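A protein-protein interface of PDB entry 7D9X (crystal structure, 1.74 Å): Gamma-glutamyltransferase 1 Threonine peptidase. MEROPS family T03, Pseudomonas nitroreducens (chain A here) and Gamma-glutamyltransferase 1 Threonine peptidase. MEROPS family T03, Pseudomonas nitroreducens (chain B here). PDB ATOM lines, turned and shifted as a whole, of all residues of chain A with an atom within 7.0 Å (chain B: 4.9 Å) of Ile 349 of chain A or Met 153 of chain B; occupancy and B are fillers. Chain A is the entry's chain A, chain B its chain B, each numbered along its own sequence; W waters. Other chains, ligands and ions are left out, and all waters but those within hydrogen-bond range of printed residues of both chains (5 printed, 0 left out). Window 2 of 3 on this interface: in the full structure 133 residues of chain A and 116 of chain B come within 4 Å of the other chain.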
ATOM      1  N   ALA A 297      25.122 -13.307   4.546  1.00  0.00           N
ATOM      2  CA  ALA A 297      25.661 -12.230   5.368  1.00  0.00           C
ATOM      3  C   ALA A 297      25.222 -10.865   4.842  1.00  0.00           C
ATOM      4  O   ALA A 297      25.042  -9.923   5.623  1.00  0.00           O
ATOM      5  CB  ALA A 297      27.190 -12.323   5.430  1.00  0.00           C
ATOM      6  N   LYS A 298      25.068 -10.733   3.523  1.00  0.00           N
ATOM      7  CA  LYS A 298      24.583  -9.479   2.956  1.00  0.00           C
ATOM      8  C   LYS A 298      23.136  -9.216   3.354  1.00  0.00           C
ATOM      9  O   LYS A 298      22.767  -8.087   3.707  1.00  0.00           O
ATOM     10  CB  LYS A 298      24.716  -9.527   1.433  1.00  0.00           C
ATOM     11  CG  LYS A 298      24.174  -8.316   0.706  1.00  0.00           C
ATOM     12  CD  LYS A 298      24.973  -7.072   1.011  1.00  0.00           C
ATOM     13  CE  LYS A 298      24.430  -5.881   0.223  1.00  0.00           C
ATOM     14  NZ  LYS A 298      24.548  -6.080  -1.248  1.00  0.00           N
ATOM     15  N   HIS A 301      23.162  -8.298   7.011  1.00  0.00           N
ATOM     16  CA  HIS A 301      23.700  -6.957   7.201  1.00  0.00           C
ATOM     17  C   HIS A 301      22.682  -5.889   6.815  1.00  0.00           C
ATOM     18  O   HIS A 301      22.541  -4.872   7.505  1.00  0.00           O
ATOM     19  CB  HIS A 301      24.977  -6.750   6.380  1.00  0.00           C
ATOM     20  CG  HIS A 301      25.331  -5.308   6.209  1.00  0.00           C
ATOM     21  ND1 HIS A 301      25.832  -4.535   7.239  1.00  0.00           N
ATOM     22  CD2 HIS A 301      25.234  -4.488   5.134  1.00  0.00           C
ATOM     23  CE1 HIS A 301      26.026  -3.304   6.804  1.00  0.00           C
ATOM     24  NE2 HIS A 301      25.679  -3.251   5.528  1.00  0.00           N
ATOM     25  N   LEU A 302      21.968  -6.090   5.706  1.00  0.00           N
ATOM     26  CA  LEU A 302      21.007  -5.081   5.270  1.00  0.00           C
ATOM     27  C   LEU A 302      19.862  -4.950   6.276  1.00  0.00           C
ATOM     28  O   LEU A 302      19.418  -3.838   6.589  1.00  0.00           O
ATOM     29  CB  LEU A 302      20.453  -5.434   3.889  1.00  0.00           C
ATOM     30  CG  LEU A 302      21.392  -5.130   2.698  1.00  0.00           C
ATOM     31  CD1 LEU A 302      20.901  -5.918   1.475  1.00  0.00           C
ATOM     32  CD2 LEU A 302      21.446  -3.640   2.392  1.00  0.00           C
ATOM     33  N   GLU A 305      21.126  -2.964   9.112  1.00  0.00           N
ATOM     34  CA  GLU A 305      21.238  -1.552   8.777  1.00  0.00           C
ATOM     35  C   GLU A 305      19.898  -0.846   8.887  1.00  0.00           C
ATOM     36  O   GLU A 305      19.836   0.311   9.324  1.00  0.00           O
ATOM     37  CB  GLU A 305      21.806  -1.383   7.363  1.00  0.00           C
ATOM     38  CG  GLU A 305      23.317  -1.422   7.276  1.00  0.00           C
ATOM     39  CD  GLU A 305      23.978  -0.160   7.848  1.00  0.00           C
ATOM     40  OE1 GLU A 305      23.662   0.948   7.377  1.00  0.00           O
ATOM     41  OE2 GLU A 305      24.791  -0.293   8.777  1.00  0.00           O
ATOM     42  N   LYS A 308      18.886  -0.617  12.657  1.00  0.00           N
ATOM     43  CA  LYS A 308      19.546   0.501  13.314  1.00  0.00           C
ATOM     44  C   LYS A 308      18.643   1.729  13.370  1.00  0.00           C
ATOM     45  O   LYS A 308      18.476   2.341  14.428  1.00  0.00           O
ATOM     46  CB  LYS A 308      20.839   0.836  12.572  1.00  0.00           C
ATOM     47  CG  LYS A 308      22.021  -0.014  12.970  1.00  0.00           C
ATOM     48  CD  LYS A 308      23.327   0.513  12.309  1.00  0.00           C
ATOM     49  CE  LYS A 308      24.518   0.230  13.180  1.00  0.00           C
ATOM     50  NZ  LYS A 308      24.787  -1.219  13.368  1.00  0.00           N
ATOM     51  N   ARG A 309      18.061   2.115  12.231  1.00  0.00           N
ATOM     52  CA  ARG A 309      17.280   3.346  12.183  1.00  0.00           C
ATOM     53  C   ARG A 309      15.954   3.179  12.912  1.00  0.00           C
ATOM     54  O   ARG A 309      15.460   4.114  13.559  1.00  0.00           O
ATOM     55  CB  ARG A 309      17.038   3.754  10.734  1.00  0.00           C
ATOM     56  CG  ARG A 309      18.186   4.563  10.110  1.00  0.00           C
ATOM     57  CD  ARG A 309      19.304   3.650   9.682  1.00  0.00           C
ATOM     58  NE  ARG A 309      20.521   4.402   9.340  1.00  0.00           N
ATOM     59  CZ  ARG A 309      21.648   3.846   8.923  1.00  0.00           C
ATOM     60  NH1 ARG A 309      21.718   2.525   8.775  1.00  0.00           N
ATOM     61  NH2 ARG A 309      22.712   4.606   8.649  1.00  0.00           N
ATOM     62  N   ASN A 345      23.529   1.538   4.550  1.00  0.00           N
ATOM     63  CA  ASN A 345      24.806   1.299   3.898  1.00  0.00           C
ATOM     64  C   ASN A 345      24.882  -0.166   3.502  1.00  0.00           C
ATOM     65  O   ASN A 345      25.050  -1.028   4.382  1.00  0.00           O
ATOM     66  CB  ASN A 345      25.963   1.669   4.830  1.00  0.00           C
ATOM     67  CG  ASN A 345      27.327   1.593   4.153  1.00  0.00           C
ATOM     68  OD1 ASN A 345      27.548   0.806   3.228  1.00  0.00           O
ATOM     69  ND2 ASN A 345      28.251   2.424   4.614  1.00  0.00           N
ATOM     70  N   PRO A 346      24.785  -0.502   2.211  1.00  0.00           N
ATOM     71  CA  PRO A 346      24.743  -1.926   1.835  1.00  0.00           C
ATOM     72  C   PRO A 346      26.076  -2.637   1.913  1.00  0.00           C
ATOM     73  O   PRO A 346      26.089  -3.874   1.921  1.00  0.00           O
ATOM     74  CB  PRO A 346      24.203  -1.903   0.394  1.00  0.00           C
ATOM     75  CG  PRO A 346      24.584  -0.539  -0.123  1.00  0.00           C
ATOM     76  CD  PRO A 346      24.504   0.389   1.072  1.00  0.00           C
ATOM     77  N   ASP A 347      27.199  -1.917   1.984  1.00  0.00           N
ATOM     78  CA  ASP A 347      28.501  -2.564   1.933  1.00  0.00           C
ATOM     79  C   ASP A 347      29.251  -2.571   3.258  1.00  0.00           C
ATOM     80  O   ASP A 347      30.201  -3.352   3.399  1.00  0.00           O
ATOM     81  CB  ASP A 347      29.385  -1.890   0.871  1.00  0.00           C
ATOM     82  CG  ASP A 347      28.780  -1.961  -0.517  1.00  0.00           C
ATOM     83  OD1 ASP A 347      28.483  -3.092  -0.973  1.00  0.00           O
ATOM     84  OD2 ASP A 347      28.593  -0.891  -1.149  1.00  0.00           O
ATOM     85  N   ALA A 348      28.855  -1.744   4.225  1.00  0.00           N
ATOM     86  CA  ALA A 348      29.568  -1.680   5.488  1.00  0.00           C
ATOM     87  C   ALA A 348      28.629  -1.201   6.581  1.00  0.00           C
ATOM     88  O   ALA A 348      27.580  -0.609   6.311  1.00  0.00           O
ATOM     89  CB  ALA A 348      30.792  -0.753   5.408  1.00  0.00           C
ATOM     90  N   ILE A 349      29.049  -1.433   7.828  1.00  0.00           N
ATOM     91  CA  ILE A 349      28.255  -1.032   8.990  1.00  0.00           C
ATOM     92  C   ILE A 349      28.287   0.485   9.114  1.00  0.00           C
ATOM     93  O   ILE A 349      29.362   1.104   9.087  1.00  0.00           O
ATOM     94  CB  ILE A 349      28.800  -1.694  10.267  1.00  0.00           C
ATOM     95  CG1 ILE A 349      28.872  -3.212  10.091  1.00  0.00           C
ATOM     96  CG2 ILE A 349      27.974  -1.294  11.465  1.00  0.00           C
ATOM     97  CD1 ILE A 349      29.371  -3.957  11.314  1.00  0.00           C
ATOM     98  N   SER A 350      27.110   1.090   9.253  1.00  0.00           N
ATOM     99  CA  SER A 350      27.027   2.507   9.567  1.00  0.00           C
ATOM    100  C   SER A 350      27.499   2.753  10.997  1.00  0.00           C
ATOM    101  O   SER A 350      27.360   1.899  11.878  1.00  0.00           O
ATOM    102  CB  SER A 350      25.601   3.011   9.400  1.00  0.00           C
ATOM    103  OG  SER A 350      25.165   2.827   8.070  1.00  0.00           O
ATOM    104  N   ALA A 351      28.087   3.932  11.216  1.00  0.00           N
ATOM    105  CA  ALA A 351      28.629   4.268  12.527  1.00  0.00           C
ATOM    106  C   ALA A 351      27.493   4.404  13.532  1.00  0.00           C
ATOM    107  O   ALA A 351      26.636   5.283  13.392  1.00  0.00           O
ATOM    108  CB  ALA A 351      29.444   5.561  12.454  1.00  0.00           C
ATOM    109  N   THR A 352      27.506   3.550  14.556  1.00  0.00           N
ATOM    110  CA  THR A 352      26.388   3.493  15.498  1.00  0.00           C
ATOM    111  C   THR A 352      26.090   4.869  16.087  1.00  0.00           C
ATOM    112  O   THR A 352      24.940   5.318  16.110  1.00  0.00           O
ATOM    113  CB  THR A 352      26.706   2.497  16.610  1.00  0.00           C
ATOM    114  OG1 THR A 352      26.726   1.169  16.073  1.00  0.00           O
ATOM    115  CG2 THR A 352      25.679   2.588  17.743  1.00  0.00           C
ATOM    116  N   ASP B 132      26.433  -2.836  17.146  1.00  0.00           N
ATOM    117  CA  ASP B 132      26.827  -3.808  16.127  1.00  0.00           C
ATOM    118  C   ASP B 132      26.776  -5.237  16.649  1.00  0.00           C
ATOM    119  O   ASP B 132      27.578  -6.094  16.271  1.00  0.00           O
ATOM    120  CB  ASP B 132      28.214  -3.467  15.581  1.00  0.00           C
ATOM    121  CG  ASP B 132      28.275  -2.079  14.979  1.00  0.00           C
ATOM    122  OD1 ASP B 132      27.207  -1.543  14.624  1.00  0.00           O
ATOM    123  OD2 ASP B 132      29.392  -1.511  14.865  1.00  0.00           O
ATOM    124  N   GLU B 149      31.775 -14.177   7.842  1.00  0.00           N
ATOM    125  CA  GLU B 149      31.636 -12.968   7.044  1.00  0.00           C
ATOM    126  C   GLU B 149      31.071 -11.832   7.882  1.00  0.00           C
ATOM    127  O   GLU B 149      31.516 -10.685   7.760  1.00  0.00           O
ATOM    128  CB  GLU B 149      30.752 -13.246   5.826  1.00  0.00           C
ATOM    129  CG  GLU B 149      31.339 -14.310   4.890  1.00  0.00           C
ATOM    130  CD  GLU B 149      30.396 -14.724   3.770  1.00  0.00           C
ATOM    131  OE1 GLU B 149      30.836 -14.744   2.602  1.00  0.00           O
ATOM    132  OE2 GLU B 149      29.219 -15.021   4.045  1.00  0.00           O
ATOM    133  N   LEU B 150      30.094 -12.128   8.749  1.00  0.00           N
ATOM    134  CA  LEU B 150      29.540 -11.082   9.602  1.00  0.00           C
ATOM    135  C   LEU B 150      30.567 -10.617  10.626  1.00  0.00           C
ATOM    136  O   LEU B 150      30.752  -9.411  10.829  1.00  0.00           O
ATOM    137  CB  LEU B 150      28.271 -11.585  10.287  1.00  0.00           C
ATOM    138  CG  LEU B 150      27.055 -11.676   9.354  1.00  0.00           C
ATOM    139  CD1 LEU B 150      25.946 -12.484  10.025  1.00  0.00           C
ATOM    140  CD2 LEU B 150      26.551 -10.286   8.955  1.00  0.00           C
ATOM    141  N   LYS B 151      31.230 -11.568  11.296  1.00  0.00           N
ATOM    142  CA  LYS B 151      32.321 -11.224  12.208  1.00  0.00           C
ATOM    143  C   LYS B 151      33.357 -10.342  11.515  1.00  0.00           C
ATOM    144  O   LYS B 151      33.853  -9.363  12.090  1.00  0.00           O
ATOM    145  CB  LYS B 151      32.976 -12.504  12.726  1.00  0.00           C
ATOM    146  CG  LYS B 151      32.286 -13.163  13.906  1.00  0.00           C
ATOM    147  CD  LYS B 151      32.905 -14.537  14.208  1.00  0.00           C
ATOM    148  CE  LYS B 151      32.321 -15.150  15.472  1.00  0.00           C
ATOM    149  N   ALA B 152      33.688 -10.670  10.262  1.00  0.00           N
ATOM    150  CA  ALA B 152      34.721  -9.918   9.553  1.00  0.00           C
ATOM    151  C   ALA B 152      34.270  -8.498   9.226  1.00  0.00           C
ATOM    152  O   ALA B 152      35.111  -7.607   9.052  1.00  0.00           O
ATOM    153  CB  ALA B 152      35.115 -10.652   8.265  1.00  0.00           C
ATOM    154  N   MET B 153      32.959  -8.267   9.123  1.00  0.00           N
ATOM    155  CA  MET B 153      32.452  -6.930   8.854  1.00  0.00           C
ATOM    156  C   MET B 153      32.520  -6.020  10.070  1.00  0.00           C
ATOM    157  O   MET B 153      32.334  -4.807   9.917  1.00  0.00           O
ATOM    158  CB  MET B 153      30.983  -6.983   8.405  1.00  0.00           C
ATOM    159  CG  MET B 153      30.731  -7.702   7.117  1.00  0.00           C
ATOM    160  SD  MET B 153      28.974  -7.575   6.707  1.00  0.00           S
ATOM    161  CE  MET B 153      28.817  -5.832   6.329  1.00  0.00           C
ATOM    162  N   GLY B 154      32.746  -6.576  11.257  1.00  0.00           N
ATOM    163  CA  GLY B 154      32.734  -5.820  12.487  1.00  0.00           C
ATOM    164  C   GLY B 154      31.596  -6.132  13.441  1.00  0.00           C
ATOM    165  O   GLY B 154      31.467  -5.454  14.477  1.00  0.00           O
ATOM    166  N   TYR B 155      30.776  -7.130  13.141  1.00  0.00           N
ATOM    167  CA  TYR B 155      29.652  -7.459  14.004  1.00  0.00           C
ATOM    168  C   TYR B 155      30.074  -8.405  15.125  1.00  0.00           C
ATOM    169  O   TYR B 155      30.934  -9.276  14.944  1.00  0.00           O
ATOM    170  CB  TYR B 155      28.509  -8.109  13.210  1.00  0.00           C
ATOM    171  CG  TYR B 155      27.666  -7.172  12.375  1.00  0.00           C
ATOM    172  CD1 TYR B 155      26.869  -6.193  12.968  1.00  0.00           C
ATOM    173  CD2 TYR B 155      27.635  -7.289  10.981  1.00  0.00           C
ATOM    174  CE1 TYR B 155      26.087  -5.335  12.193  1.00  0.00           C
ATOM    175  CE2 TYR B 155      26.852  -6.445  10.212  1.00  0.00           C
ATOM    176  CZ  TYR B 155      26.080  -5.470  10.822  1.00  0.00           C
ATOM    177  OH  TYR B 155      25.312  -4.628  10.027  1.00  0.00           O
HETATM  178  O   HOH W   1      28.759   0.748  14.242  1.00  0.00           O
HETATM  179  O   HOH W   2      24.221  -2.289  10.744  1.00  0.00           O
HETATM  180  O   HOH W   3      32.004  -2.966   8.346  1.00  0.00           O
HETATM  181  O   HOH W   4      24.781  -0.676  16.351  1.00  0.00           O
HETATM  182  O   HOH W   5      26.877 -15.061   2.968  1.00  0.00           O
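The side-chain carboxylate (OD1) of Asp 132 of chain B is in hydrogen-bond range of the side-chain hydroxyl (OG1) of Thr 352 of chain A (3.1 Å). OD1 of Asp 132 of chain B lies within salt-bridge range of NZ of Lys 308 of chain A (2.7 Å). OH of Tyr 155 of chain B sits at hydrogen-bond distance from ND1 of His 301 of chain A (2.8 Å).
O of Asn 345 of chain A sits at hydrogen-bond distance from NE2 of His 301 of chain A, 2.6 Å away. The backbone carbonyl oxygen (O) of Leu 150 of chain B lies within hydrogen-bond range of the backbone NH (N) of Tyr 155 of chain B (3.2 Å). NE2 of His 301 of chain A sits close to O of Ala 348 of chain A (3.3 Å).
Ala 297 of chain A touches Glu 149 of chain B (CB to OE2, 3.6 Å). Ala 297 of chain A touches Leu 150 of chain B. His 301 of chain A touches Met 153 of chain B. Asp 132 of chain B touches Ile 349 of chain A. Ile 349 of chain A touches Met 153 of chain B (CD1 to O, 3.4 Å). Gly 154 of chain B touches Ile 349 of chain A (C to CD1, 3.8 Å). CD1 of Ile 349 of chain A touches CZ of Tyr 155 of chain B (3.7 Å).
Ile 349 of chain A touches four residues of chain B. Met 153 of chain B touches just these residues of chain A: His 301 and Ile 349. Of the printed residues of chain B, Ala 297 of chain A touches Glu 149 and Leu 150. Of the printed residues of chain A, Leu 150 of chain B touches Ala 297 (3.7 Å). Of the printed residues of chain A, Tyr 155 of chain B touches His 301 (2.8 Å) and Ile 349 (3.7 Å). Of the printed residues of chain A, Gly 154 of chain B touches Ile 349. Of the printed residues of chain A, Asp 132 of chain B touches Lys 308, Ile 349 and Thr 352. Pro 346 of chain A touches none of the printed residues of chain B. The nearest printed residue of chain B that does not touch Ile 349 of chain A is Leu 150 of chain B (5.6 Å). The nearest printed residue of chain A that does not touch Gly 154 of chain B is Lys 308 of chain A (8.0 Å).
Of the 8 printed residues of chain B, 6 touch a printed residue of chain A. Of the 15 printed residues of chain A, 5 touch a printed residue of chain B. Hydrophobic or aromatic side chains of chain A within 4 Å of the printed part of chain B: Ala 297, His 301 and Ile 349.
Water W1 lies within hydrogen-bond range of the side-chain carboxylate (OD2) of Asp 132 of chain B (2.4 Å), the side-chain hydroxyl (OG1) of Thr 352 of chain A (2.8 Å) and the backbone carbonyl oxygen (O) of Ser 350 of chain A (3.0 Å). Water W3 bridges O of Met 153 of chain B (2.4 Å) and N of Ile 349 of chain A (3.4 Å). Water W5 lies within hydrogen-bond range of the side-chain carboxylate (OE2) of Glu 149 of chain B and the backbone NH (N) of Ala 297 of chain A. Water W2 lies within hydrogen-bond range of OH of Tyr 155 of chain B (2.7 Å), OE2 of Glu 305 of chain A (2.9 Å) and NZ of Lys 308 of chain A (2.9 Å). Water W4 lies within hydrogen-bond range of the side-chain hydroxyl of Thr 352 of chain A (2.7 Å), the backbone NH of Asp 132 of chain B (2.8 Å) and the side-chain amino group of Lys 308 of chain A (3.0 Å).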
